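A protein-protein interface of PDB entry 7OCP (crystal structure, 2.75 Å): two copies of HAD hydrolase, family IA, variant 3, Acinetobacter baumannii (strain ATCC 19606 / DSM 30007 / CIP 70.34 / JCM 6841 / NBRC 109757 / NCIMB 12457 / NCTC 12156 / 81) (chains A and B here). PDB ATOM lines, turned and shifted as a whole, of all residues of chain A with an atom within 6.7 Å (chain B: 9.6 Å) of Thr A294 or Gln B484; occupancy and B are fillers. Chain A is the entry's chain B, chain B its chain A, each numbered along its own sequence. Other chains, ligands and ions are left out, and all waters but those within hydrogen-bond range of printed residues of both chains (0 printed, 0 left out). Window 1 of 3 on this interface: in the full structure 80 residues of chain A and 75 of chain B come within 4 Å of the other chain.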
ATOM      1  N   ALA A 288     -15.939 -12.958  27.586  1.00  0.00           N
ATOM      2  CA  ALA A 288     -15.451 -12.518  26.255  1.00  0.00           C
ATOM      3  C   ALA A 288     -16.538 -11.709  25.537  1.00  0.00           C
ATOM      4  O   ALA A 288     -16.225 -10.603  25.056  1.00  0.00           O
ATOM      5  CB  ALA A 288     -15.021 -13.708  25.432  1.00  0.00           C
ATOM      6  N   VAL A 289     -17.760 -12.243  25.465  1.00  0.00           N
ATOM      7  CA  VAL A 289     -18.918 -11.612  24.759  1.00  0.00           C
ATOM      8  C   VAL A 289     -19.294 -10.316  25.487  1.00  0.00           C
ATOM      9  O   VAL A 289     -19.477  -9.292  24.802  1.00  0.00           O
ATOM     10  CB  VAL A 289     -20.121 -12.572  24.657  1.00  0.00           C
ATOM     11  CG1 VAL A 289     -21.369 -11.870  24.140  1.00  0.00           C
ATOM     12  CG2 VAL A 289     -19.804 -13.785  23.798  1.00  0.00           C
ATOM     13  N   ASN A 290     -19.401 -10.368  26.820  1.00  0.00           N
ATOM     14  CA  ASN A 290     -19.779  -9.219  27.688  1.00  0.00           C
ATOM     15  C   ASN A 290     -18.727  -8.108  27.573  1.00  0.00           C
ATOM     16  O   ASN A 290     -19.111  -6.926  27.683  1.00  0.00           O
ATOM     17  CB  ASN A 290     -19.969  -9.651  29.145  1.00  0.00           C
ATOM     18  CG  ASN A 290     -21.173 -10.548  29.350  1.00  0.00           C
ATOM     19  OD1 ASN A 290     -22.001 -10.707  28.455  1.00  0.00           O
ATOM     20  ND2 ASN A 290     -21.280 -11.139  30.529  1.00  0.00           N
ATOM     21  N   ALA A 291     -17.457  -8.474  27.360  1.00  0.00           N
ATOM     22  CA  ALA A 291     -16.312  -7.545  27.212  1.00  0.00           C
ATOM     23  C   ALA A 291     -16.397  -6.819  25.864  1.00  0.00           C
ATOM     24  O   ALA A 291     -16.276  -5.582  25.859  1.00  0.00           O
ATOM     25  CB  ALA A 291     -15.006  -8.291  27.348  1.00  0.00           C
ATOM     26  N   PHE A 292     -16.584  -7.568  24.772  1.00  0.00           N
ATOM     27  CA  PHE A 292     -16.690  -7.045  23.382  1.00  0.00           C
ATOM     28  C   PHE A 292     -18.043  -6.353  23.178  1.00  0.00           C
ATOM     29  O   PHE A 292     -18.102  -5.387  22.399  1.00  0.00           O
ATOM     30  CB  PHE A 292     -16.508  -8.165  22.353  1.00  0.00           C
ATOM     31  CG  PHE A 292     -15.097  -8.343  21.855  1.00  0.00           C
ATOM     32  CD1 PHE A 292     -14.176  -9.089  22.573  1.00  0.00           C
ATOM     33  CD2 PHE A 292     -14.691  -7.767  20.661  1.00  0.00           C
ATOM     34  CE1 PHE A 292     -12.879  -9.252  22.110  1.00  0.00           C
ATOM     35  CE2 PHE A 292     -13.393  -7.931  20.198  1.00  0.00           C
ATOM     36  CZ  PHE A 292     -12.490  -8.673  20.923  1.00  0.00           C
ATOM     37  N   GLY A 293     -19.094  -6.850  23.840  1.00  0.00           N
ATOM     38  CA  GLY A 293     -20.481  -6.369  23.690  1.00  0.00           C
ATOM     39  C   GLY A 293     -21.205  -7.076  22.555  1.00  0.00           C
ATOM     40  O   GLY A 293     -22.437  -6.924  22.457  1.00  0.00           O
ATOM     41  N   THR A 294     -20.464  -7.819  21.727  1.00  0.00           N
ATOM     42  CA  THR A 294     -20.974  -8.576  20.553  1.00  0.00           C
ATOM     43  C   THR A 294     -20.114  -9.826  20.338  1.00  0.00           C
ATOM     44  O   THR A 294     -18.984  -9.871  20.869  1.00  0.00           O
ATOM     45  CB  THR A 294     -20.949  -7.718  19.283  1.00  0.00           C
ATOM     46  OG1 THR A 294     -19.602  -7.298  19.065  1.00  0.00           O
ATOM     47  CG2 THR A 294     -21.853  -6.507  19.362  1.00  0.00           C
ATOM     48  N   TYR A 295     -20.641 -10.795  19.588  1.00  0.00           N
ATOM     49  CA  TYR A 295     -19.875 -11.909  18.972  1.00  0.00           C
ATOM     50  C   TYR A 295     -20.330 -12.056  17.516  1.00  0.00           C
ATOM     51  O   TYR A 295     -21.395 -11.509  17.164  1.00  0.00           O
ATOM     52  CB  TYR A 295     -20.040 -13.202  19.774  1.00  0.00           C
ATOM     53  CG  TYR A 295     -21.379 -13.876  19.621  1.00  0.00           C
ATOM     54  CD1 TYR A 295     -21.615 -14.772  18.591  1.00  0.00           C
ATOM     55  CD2 TYR A 295     -22.412 -13.620  20.507  1.00  0.00           C
ATOM     56  CE1 TYR A 295     -22.843 -15.395  18.443  1.00  0.00           C
ATOM     57  CE2 TYR A 295     -23.645 -14.235  20.374  1.00  0.00           C
ATOM     58  CZ  TYR A 295     -23.862 -15.126  19.338  1.00  0.00           C
ATOM     59  OH  TYR A 295     -25.076 -15.733  19.208  1.00  0.00           O
ATOM     60  N   SER A 296     -19.542 -12.766  16.706  1.00  0.00           N
ATOM     61  CA  SER A 296     -19.767 -12.948  15.249  1.00  0.00           C
ATOM     62  C   SER A 296     -19.838 -14.440  14.902  1.00  0.00           C
ATOM     63  O   SER A 296     -19.046 -15.220  15.468  1.00  0.00           O
ATOM     64  CB  SER A 296     -18.702 -12.245  14.454  1.00  0.00           C
ATOM     65  OG  SER A 296     -18.834 -10.837  14.573  1.00  0.00           O
ATOM     66  N   ARG A 307     -22.267 -10.233  12.694  1.00  0.00           N
ATOM     67  CA  ARG A 307     -22.220  -9.618  14.048  1.00  0.00           C
ATOM     68  C   ARG A 307     -23.601  -9.744  14.705  1.00  0.00           C
ATOM     69  O   ARG A 307     -24.590  -9.308  14.083  1.00  0.00           O
ATOM     70  CB  ARG A 307     -21.775  -8.154  13.956  1.00  0.00           C
ATOM     71  CG  ARG A 307     -21.709  -7.435  15.296  1.00  0.00           C
ATOM     72  CD  ARG A 307     -21.138  -6.032  15.203  1.00  0.00           C
ATOM     73  NE  ARG A 307     -19.684  -6.012  15.306  1.00  0.00           N
ATOM     74  CZ  ARG A 307     -18.832  -5.989  14.281  1.00  0.00           C
ATOM     75  NH1 ARG A 307     -17.531  -5.975  14.515  1.00  0.00           N
ATOM     76  NH2 ARG A 307     -19.270  -5.984  13.032  1.00  0.00           N
ATOM     77  N   ILE A 308     -23.651 -10.319  15.914  1.00  0.00           N
ATOM     78  CA  ILE A 308     -24.882 -10.486  16.746  1.00  0.00           C
ATOM     79  C   ILE A 308     -24.846  -9.444  17.872  1.00  0.00           C
ATOM     80  O   ILE A 308     -24.002  -9.586  18.777  1.00  0.00           O
ATOM     81  CB  ILE A 308     -24.983 -11.923  17.301  1.00  0.00           C
ATOM     82  CG1 ILE A 308     -24.877 -12.982  16.199  1.00  0.00           C
ATOM     83  CG2 ILE A 308     -26.250 -12.097  18.126  1.00  0.00           C
ATOM     84  CD1 ILE A 308     -25.995 -12.943  15.179  1.00  0.00           C
ATOM     85  N   GLU A 309     -25.734  -8.444  17.813  1.00  0.00           N
ATOM     86  CA  GLU A 309     -25.783  -7.297  18.761  1.00  0.00           C
ATOM     87  C   GLU A 309     -26.853  -7.548  19.831  1.00  0.00           C
ATOM     88  O   GLU A 309     -27.719  -8.420  19.611  1.00  0.00           O
ATOM     89  CB  GLU A 309     -26.078  -5.998  18.009  1.00  0.00           C
ATOM     90  CG  GLU A 309     -25.164  -5.759  16.820  1.00  0.00           C
ATOM     91  CD  GLU A 309     -25.290  -4.392  16.166  1.00  0.00           C
ATOM     92  OE1 GLU A 309     -26.134  -3.589  16.616  1.00  0.00           O
ATOM     93  OE2 GLU A 309     -24.539  -4.133  15.204  1.00  0.00           O
ATOM     94  N   ASN A 310     -26.781  -6.803  20.940  1.00  0.00           N
ATOM     95  CA  ASN A 310     -27.776  -6.792  22.049  1.00  0.00           C
ATOM     96  C   ASN A 310     -27.763  -8.146  22.770  1.00  0.00           C
ATOM     97  O   ASN A 310     -28.857  -8.676  23.050  1.00  0.00           O
ATOM     98  CB  ASN A 310     -29.180  -6.443  21.544  1.00  0.00           C
ATOM     99  CG  ASN A 310     -29.217  -5.175  20.717  1.00  0.00           C
ATOM    100  OD1 ASN A 310     -28.579  -4.184  21.062  1.00  0.00           O
ATOM    101  ND2 ASN A 310     -29.963  -5.199  19.625  1.00  0.00           N
ATOM    102  N   MET A 311     -26.570  -8.672  23.069  1.00  0.00           N
ATOM    103  CA  MET A 311     -26.376  -9.971  23.768  1.00  0.00           C
ATOM    104  C   MET A 311     -26.065  -9.716  25.248  1.00  0.00           C
ATOM    105  O   MET A 311     -25.297  -8.776  25.542  1.00  0.00           O
ATOM    106  CB  MET A 311     -25.230 -10.772  23.145  1.00  0.00           C
ATOM    107  CG  MET A 311     -25.562 -11.366  21.786  1.00  0.00           C
ATOM    108  SD  MET A 311     -26.950 -12.537  21.811  1.00  0.00           S
ATOM    109  CE  MET A 311     -26.408 -13.704  23.059  1.00  0.00           C
ATOM    110  N   LEU A 483     -13.052  -1.781  17.126  1.00  0.00           N
ATOM    111  CA  LEU A 483     -14.148  -2.781  16.979  1.00  0.00           C
ATOM    112  C   LEU A 483     -14.852  -2.633  15.621  1.00  0.00           C
ATOM    113  O   LEU A 483     -15.644  -3.536  15.284  1.00  0.00           O
ATOM    114  CB  LEU A 483     -15.147  -2.613  18.127  1.00  0.00           C
ATOM    115  CG  LEU A 483     -14.596  -2.874  19.530  1.00  0.00           C
ATOM    116  CD1 LEU A 483     -15.673  -2.643  20.580  1.00  0.00           C
ATOM    117  CD2 LEU A 483     -14.031  -4.281  19.646  1.00  0.00           C
ATOM    118  N   MET A 486     -12.315  -5.168  14.051  1.00  0.00           N
ATOM    119  CA  MET A 486     -12.107  -6.311  14.984  1.00  0.00           C
ATOM    120  C   MET A 486     -13.457  -6.953  15.320  1.00  0.00           C
ATOM    121  O   MET A 486     -14.364  -6.218  15.751  1.00  0.00           O
ATOM    122  CB  MET A 486     -11.430  -5.837  16.275  1.00  0.00           C
ATOM    123  CG  MET A 486     -10.951  -6.965  17.167  1.00  0.00           C
ATOM    124  SD  MET A 486      -9.899  -6.373  18.520  1.00  0.00           S
ATOM    125  CE  MET A 486      -8.381  -6.033  17.632  1.00  0.00           C
ATOM    126  N   ASP A 487     -13.572  -8.272  15.121  1.00  0.00           N
ATOM    127  CA  ASP A 487     -14.765  -9.099  15.457  1.00  0.00           C
ATOM    128  C   ASP A 487     -14.356 -10.169  16.475  1.00  0.00           C
ATOM    129  O   ASP A 487     -13.158 -10.494  16.532  1.00  0.00           O
ATOM    130  CB  ASP A 487     -15.355  -9.761  14.208  1.00  0.00           C
ATOM    131  CG  ASP A 487     -16.237  -8.850  13.371  1.00  0.00           C
ATOM    132  OD1 ASP A 487     -15.745  -8.343  12.341  1.00  0.00           O
ATOM    133  OD2 ASP A 487     -17.415  -8.675  13.741  1.00  0.00           O
ATOM    134  N   LEU A 488     -15.317 -10.691  17.243  1.00  0.00           N
ATOM    135  CA  LEU A 488     -15.126 -11.860  18.145  1.00  0.00           C
ATOM    136  C   LEU A 488     -15.794 -13.084  17.508  1.00  0.00           C
ATOM    137  O   LEU A 488     -17.033 -13.187  17.579  1.00  0.00           O
ATOM    138  CB  LEU A 488     -15.716 -11.546  19.524  1.00  0.00           C
ATOM    139  CG  LEU A 488     -15.517 -12.627  20.587  1.00  0.00           C
ATOM    140  CD1 LEU A 488     -14.046 -12.781  20.940  1.00  0.00           C
ATOM    141  CD2 LEU A 488     -16.333 -12.318  21.833  1.00  0.00           C
ATOM    142  N   LEU A 490     -16.796 -16.816  17.456  1.00  0.00           N
ATOM    143  CA  LEU A 490     -17.092 -17.886  18.447  1.00  0.00           C
ATOM    144  C   LEU A 490     -17.712 -19.118  17.773  1.00  0.00           C
ATOM    145  O   LEU A 490     -17.734 -20.180  18.429  1.00  0.00           O
ATOM    146  CB  LEU A 490     -18.039 -17.327  19.516  1.00  0.00           C
ATOM    147  CG  LEU A 490     -17.489 -16.178  20.359  1.00  0.00           C
ATOM    148  CD1 LEU A 490     -18.484 -15.779  21.435  1.00  0.00           C
ATOM    149  CD2 LEU A 490     -16.150 -16.543  20.985  1.00  0.00           C
ATOM    150  N   PHE B 292     -16.702   9.887  17.716  1.00  0.00           N
ATOM    151  CA  PHE B 292     -17.541   8.689  17.440  1.00  0.00           C
ATOM    152  C   PHE B 292     -16.764   7.687  16.577  1.00  0.00           C
ATOM    153  O   PHE B 292     -17.036   6.473  16.685  1.00  0.00           O
ATOM    154  CB  PHE B 292     -18.852   9.081  16.748  1.00  0.00           C
ATOM    155  CG  PHE B 292     -20.032   9.250  17.670  1.00  0.00           C
ATOM    156  CD1 PHE B 292     -20.265  10.455  18.316  1.00  0.00           C
ATOM    157  CD2 PHE B 292     -20.916   8.204  17.888  1.00  0.00           C
ATOM    158  CE1 PHE B 292     -21.354  10.607  19.162  1.00  0.00           C
ATOM    159  CE2 PHE B 292     -22.003   8.358  18.734  1.00  0.00           C
ATOM    160  CZ  PHE B 292     -22.221   9.559  19.369  1.00  0.00           C
ATOM    161  N   THR B 294     -17.075   7.609  13.399  1.00  0.00           N
ATOM    162  CA  THR B 294     -18.124   7.245  12.410  1.00  0.00           C
ATOM    163  C   THR B 294     -19.257   8.277  12.468  1.00  0.00           C
ATOM    164  O   THR B 294     -19.451   8.874  13.542  1.00  0.00           O
ATOM    165  CB  THR B 294     -18.659   5.831  12.675  1.00  0.00           C
ATOM    166  OG1 THR B 294     -19.567   5.486  11.630  1.00  0.00           O
ATOM    167  CG2 THR B 294     -19.355   5.699  14.013  1.00  0.00           C
ATOM    168  N   SER B 296     -23.497   8.846  10.383  1.00  0.00           N
ATOM    169  CA  SER B 296     -24.612   8.129   9.711  1.00  0.00           C
ATOM    170  C   SER B 296     -25.407   9.088   8.818  1.00  0.00           C
ATOM    171  O   SER B 296     -25.598  10.254   9.217  1.00  0.00           O
ATOM    172  CB  SER B 296     -25.494   7.455  10.726  1.00  0.00           C
ATOM    173  OG  SER B 296     -24.760   6.488  11.463  1.00  0.00           O
ATOM    174  N   ASP B 305     -30.924   4.683   8.808  1.00  0.00           N
ATOM    175  CA  ASP B 305     -29.650   5.360   9.172  1.00  0.00           C
ATOM    176  C   ASP B 305     -28.478   4.524   8.647  1.00  0.00           C
ATOM    177  O   ASP B 305     -28.257   3.421   9.174  1.00  0.00           O
ATOM    178  CB  ASP B 305     -29.549   5.577  10.684  1.00  0.00           C
ATOM    179  CG  ASP B 305     -30.664   6.435  11.260  1.00  0.00           C
ATOM    180  OD1 ASP B 305     -31.376   7.085  10.467  1.00  0.00           O
ATOM    181  OD2 ASP B 305     -30.812   6.445  12.497  1.00  0.00           O
ATOM    182  N   ARG B 307     -24.687   3.829   8.346  1.00  0.00           N
ATOM    183  CA  ARG B 307     -23.425   4.050   9.106  1.00  0.00           C
ATOM    184  C   ARG B 307     -22.237   4.056   8.137  1.00  0.00           C
ATOM    185  O   ARG B 307     -21.969   3.003   7.527  1.00  0.00           O
ATOM    186  CB  ARG B 307     -23.244   2.959  10.166  1.00  0.00           C
ATOM    187  CG  ARG B 307     -21.969   3.080  10.991  1.00  0.00           C
ATOM    188  CD  ARG B 307     -22.212   3.590  12.397  1.00  0.00           C
ATOM    189  NE  ARG B 307     -22.950   2.625  13.203  1.00  0.00           N
ATOM    190  CZ  ARG B 307     -23.252   2.776  14.490  1.00  0.00           C
ATOM    191  NH1 ARG B 307     -23.932   1.832  15.121  1.00  0.00           N
ATOM    192  NH2 ARG B 307     -22.878   3.863  15.146  1.00  0.00           N
ATOM    193  N   HIS B 440     -25.359   5.179  30.587  1.00  0.00           N
ATOM    194  CA  HIS B 440     -24.702   3.887  30.252  1.00  0.00           C
ATOM    195  C   HIS B 440     -23.513   3.630  31.188  1.00  0.00           C
ATOM    196  O   HIS B 440     -23.310   2.457  31.552  1.00  0.00           O
ATOM    197  CB  HIS B 440     -24.286   3.871  28.773  1.00  0.00           C
ATOM    198  CG  HIS B 440     -23.490   2.671  28.382  1.00  0.00           C
ATOM    199  ND1 HIS B 440     -24.037   1.404  28.340  1.00  0.00           N
ATOM    200  CD2 HIS B 440     -22.197   2.538  28.016  1.00  0.00           C
ATOM    201  CE1 HIS B 440     -23.114   0.541  27.965  1.00  0.00           C
ATOM    202  NE2 HIS B 440     -21.976   1.214  27.760  1.00  0.00           N
ATOM    203  N   PHE B 477     -13.656  -1.258  25.984  1.00  0.00           N
ATOM    204  CA  PHE B 477     -14.751  -1.461  24.996  1.00  0.00           C
ATOM    205  C   PHE B 477     -16.118  -1.123  25.608  1.00  0.00           C
ATOM    206  O   PHE B 477     -16.948  -0.531  24.888  1.00  0.00           O
ATOM    207  CB  PHE B 477     -14.758  -2.897  24.463  1.00  0.00           C
ATOM    208  CG  PHE B 477     -13.524  -3.324  23.705  1.00  0.00           C
ATOM    209  CD1 PHE B 477     -12.823  -2.434  22.906  1.00  0.00           C
ATOM    210  CD2 PHE B 477     -13.084  -4.638  23.766  1.00  0.00           C
ATOM    211  CE1 PHE B 477     -11.696  -2.841  22.207  1.00  0.00           C
ATOM    212  CE2 PHE B 477     -11.957  -5.043  23.067  1.00  0.00           C
ATOM    213  CZ  PHE B 477     -11.266  -4.145  22.289  1.00  0.00           C
ATOM    214  N   GLN B 478     -16.348  -1.486  26.877  1.00  0.00           N
ATOM    215  CA  GLN B 478     -17.681  -1.420  27.544  1.00  0.00           C
ATOM    216  C   GLN B 478     -18.269  -0.014  27.433  1.00  0.00           C
ATOM    217  O   GLN B 478     -19.454   0.121  27.139  1.00  0.00           O
ATOM    218  CB  GLN B 478     -17.602  -1.889  28.999  1.00  0.00           C
ATOM    219  CG  GLN B 478     -18.960  -1.966  29.684  1.00  0.00           C
ATOM    220  CD  GLN B 478     -18.918  -2.767  30.963  1.00  0.00           C
ATOM    221  OE1 GLN B 478     -17.932  -2.754  31.696  1.00  0.00           O
ATOM    222  NE2 GLN B 478     -20.003  -3.470  31.244  1.00  0.00           N
ATOM    223  N   PRO B 479     -17.495   1.075  27.666  1.00  0.00           N
ATOM    224  CA  PRO B 479     -18.012   2.434  27.486  1.00  0.00           C
ATOM    225  C   PRO B 479     -18.624   2.703  26.100  1.00  0.00           C
ATOM    226  O   PRO B 479     -19.551   3.489  26.030  1.00  0.00           O
ATOM    227  CB  PRO B 479     -16.774   3.319  27.697  1.00  0.00           C
ATOM    228  CG  PRO B 479     -15.892   2.502  28.612  1.00  0.00           C
ATOM    229  CD  PRO B 479     -16.110   1.071  28.167  1.00  0.00           C
ATOM    230  N   GLY B 480     -18.103   2.049  25.053  1.00  0.00           N
ATOM    231  CA  GLY B 480     -18.531   2.230  23.650  1.00  0.00           C
ATOM    232  C   GLY B 480     -19.509   1.162  23.177  1.00  0.00           C
ATOM    233  O   GLY B 480     -19.695   1.049  21.951  1.00  0.00           O
ATOM    234  N   HIS B 481     -20.117   0.406  24.099  1.00  0.00           N
ATOM    235  CA  HIS B 481     -21.170  -0.609  23.811  1.00  0.00           C
ATOM    236  C   HIS B 481     -22.444   0.083  23.313  1.00  0.00           C
ATOM    237  O   HIS B 481     -23.190  -0.545  22.535  1.00  0.00           O
ATOM    238  CB  HIS B 481     -21.453  -1.473  25.051  1.00  0.00           C
ATOM    239  CG  HIS B 481     -20.458  -2.562  25.272  1.00  0.00           C
ATOM    240  ND1 HIS B 481     -19.244  -2.597  24.614  1.00  0.00           N
ATOM    241  CD2 HIS B 481     -20.483  -3.643  26.083  1.00  0.00           C
ATOM    242  CE1 HIS B 481     -18.569  -3.659  24.999  1.00  0.00           C
ATOM    243  NE2 HIS B 481     -19.306  -4.317  25.903  1.00  0.00           N
ATOM    244  N   ILE B 482     -22.677   1.325  23.753  1.00  0.00           N
ATOM    245  CA  ILE B 482     -23.872   2.152  23.405  1.00  0.00           C
ATOM    246  C   ILE B 482     -23.890   2.427  21.892  1.00  0.00           C
ATOM    247  O   ILE B 482     -24.996   2.610  21.349  1.00  0.00           O
ATOM    248  CB  ILE B 482     -23.900   3.452  24.243  1.00  0.00           C
ATOM    249  CG1 ILE B 482     -25.286   4.102  24.256  1.00  0.00           C
ATOM    250  CG2 ILE B 482     -22.825   4.430  23.788  1.00  0.00           C
ATOM    251  CD1 ILE B 482     -26.291   3.403  25.143  1.00  0.00           C
ATOM    252  N   LEU B 483     -22.720   2.428  21.239  1.00  0.00           N
ATOM    253  CA  LEU B 483     -22.560   2.739  19.788  1.00  0.00           C
ATOM    254  C   LEU B 483     -23.255   1.678  18.921  1.00  0.00           C
ATOM    255  O   LEU B 483     -23.480   1.970  17.730  1.00  0.00           O
ATOM    256  CB  LEU B 483     -21.068   2.828  19.443  1.00  0.00           C
ATOM    257  CG  LEU B 483     -20.294   3.965  20.112  1.00  0.00           C
ATOM    258  CD1 LEU B 483     -18.810   3.869  19.789  1.00  0.00           C
ATOM    259  CD2 LEU B 483     -20.841   5.322  19.695  1.00  0.00           C
ATOM    260  N   GLN B 484     -23.560   0.499  19.480  1.00  0.00           N
ATOM    261  CA  GLN B 484     -24.325  -0.590  18.806  1.00  0.00           C
ATOM    262  C   GLN B 484     -25.647  -0.031  18.264  1.00  0.00           C
ATOM    263  O   GLN B 484     -25.895  -0.178  17.049  1.00  0.00           O
ATOM    264  CB  GLN B 484     -24.610  -1.743  19.773  1.00  0.00           C
ATOM    265  CG  GLN B 484     -23.408  -2.639  20.045  1.00  0.00           C
ATOM    266  CD  GLN B 484     -23.715  -3.730  21.042  1.00  0.00           C
ATOM    267  OE1 GLN B 484     -24.868  -4.099  21.259  1.00  0.00           O
ATOM    268  NE2 GLN B 484     -22.674  -4.264  21.661  1.00  0.00           N
ATOM    269  N   SER B 485     -26.455   0.575  19.141  1.00  0.00           N
ATOM    270  CA  SER B 485     -27.790   1.159  18.837  1.00  0.00           C
ATOM    271  C   SER B 485     -27.765   2.673  19.086  1.00  0.00           C
ATOM    272  O   SER B 485     -28.679   3.182  19.769  1.00  0.00           O
ATOM    273  CB  SER B 485     -28.865   0.474  19.649  1.00  0.00           C
ATOM    274  OG  SER B 485     -30.154   0.971  19.316  1.00  0.00           O
ATOM    275  N   MET B 486     -26.749   3.359  18.553  1.00  0.00           N
ATOM    276  CA  MET B 486     -26.588   4.839  18.620  1.00  0.00           C
ATOM    277  C   MET B 486     -25.764   5.301  17.413  1.00  0.00           C
ATOM    278  O   MET B 486     -24.696   4.707  17.169  1.00  0.00           O
ATOM    279  CB  MET B 486     -25.883   5.267  19.911  1.00  0.00           C
ATOM    280  CG  MET B 486     -25.728   6.773  20.053  1.00  0.00           C
ATOM    281  SD  MET B 486     -24.887   7.251  21.583  1.00  0.00           S
ATOM    282  CE  MET B 486     -26.207   7.001  22.768  1.00  0.00           C
ATOM    283  N   ASP B 487     -26.251   6.323  16.702  1.00  0.00           N
ATOM    284  CA  ASP B 487     -25.640   6.865  15.457  1.00  0.00           C
ATOM    285  C   ASP B 487     -25.482   8.384  15.583  1.00  0.00           C
ATOM    286  O   ASP B 487     -26.316   9.010  16.267  1.00  0.00           O
ATOM    287  CB  ASP B 487     -26.491   6.516  14.235  1.00  0.00           C
ATOM    288  CG  ASP B 487     -26.549   5.028  13.936  1.00  0.00           C
ATOM    289  OD1 ASP B 487     -27.142   4.293  14.749  1.00  0.00           O
ATOM    290  OD2 ASP B 487     -25.995   4.616  12.894  1.00  0.00           O
ATOM    291  N   LEU B 488     -24.450   8.943  14.943  1.00  0.00           N
ATOM    292  CA  LEU B 488     -24.244  10.409  14.797  1.00  0.00           C
ATOM    293  C   LEU B 488     -24.798  10.843  13.434  1.00  0.00           C
ATOM    294  O   LEU B 488     -24.069  10.723  12.427  1.00  0.00           O
ATOM    295  CB  LEU B 488     -22.752  10.732  14.939  1.00  0.00           C
ATOM    296  CG  LEU B 488     -22.401  12.219  14.999  1.00  0.00           C
ATOM    297  CD1 LEU B 488     -22.977  12.869  16.249  1.00  0.00           C
ATOM    298  CD2 LEU B 488     -20.894  12.421  14.941  1.00  0.00           C
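NE2 of Gln B484 sits at hydrogen-bond distance from O of Gly A293 (2.8 Å). A ring nitrogen (NE2) of His B481 sits close to the backbone carbonyl oxygen (O) of Ala A291 (3.3 Å). The backbone carbonyl oxygen (O) of Asn A290 sits at hydrogen-bond distance from a ring nitrogen (NE2) of His B481, 3.2 Å away. OE1 of Glu A309 sits close to O of Gln B484 (3.4 Å). N of Asn A310 sits at hydrogen-bond distance from OE1 of Gln B484 (3.3 Å). The backbone NH of Gly A293 lies close to a ring nitrogen (NE2) of His B481, 3.3 Å away.
NH1 of Arg A307 is in hydrogen-bond range of O of Leu A483, at 3.2 Å. The backbone carbonyl oxygen of Gln B484 is in hydrogen-bond range of the guanidinium group of Arg B307 (3.4 Å). The backbone carbonyl oxygen of Phe B477 lies within hydrogen-bond range of a ring nitrogen (ND1) of His B481 (3.1 Å).
Among the printed residues, pairs that only touch across the chains: Phe A292 with His B481 (3.2 Å), Thr A294 with Gln B484 (3.3 Å), Ala A291 with Phe B477 (3.4 Å) and Leu A483 with Phe B477 (3.7 Å).
Printed residues of chain B within 4 Å of Asn A290: His B481. Of the printed residues of chain B, Ala A291 touches Phe B477 and His B481. Of chain B, only His B481 and Gln B484 come within 4 Å of Gly A293. Thr A294 touches just one residue of chain B: Gln B484. Ser A296 touches none of the printed residues of chain B. Of chain B, only Gln B484 comes within 4 Å of Glu A309. Of the printed residues of chain B, Asn A310 touches Gln B484. Printed residues of chain A within 4 Å of Phe B477: Ala A291 (3.4 Å) and Leu A483 (3.7 Å). Of the printed residues of chain A, His B481 touches Asn A290 (3.2 Å), Ala A291 (3.1 Å), Phe A292 (3.2 Å) and Gly A293 (3.2 Å). Ile B482 touches none of the printed residues of chain A. Of chain A, only Gly A293 (2.8 Å), Thr A294 (3.3 Å), Glu A309 (3.4 Å) and Asn A310 (3.3 Å) come within 4 Å of Gln B484. The nearest printed residue of chain B that does not touch Phe A292 is Phe B477 (4.2 Å).
Of the 19 printed residues of chain A, 8 touch a printed residue of chain B. Hydrophobic or aromatic side chains of chain A that line the printed part of chain B: Leu A483. Of the 18 printed residues of chain B, 3 touch a printed residue of chain A. Hydrophobic or aromatic side chains of chain B that line the printed part of chain A: Phe B477 and His B481. Among the printed residues, 10 pairs touch across the chains. Among the printed residues, no Asp or Glu carboxylate lies within 4 Å of a Lys or Arg side-chain nitrogen of the other chain.
Positions printed for both chains: 292, 294, 296, 307, 483, 486, 487 and 488. Of the 10 pairs that touch across the chains among the printed residues, none has its exchanged pair printed and touching as well.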
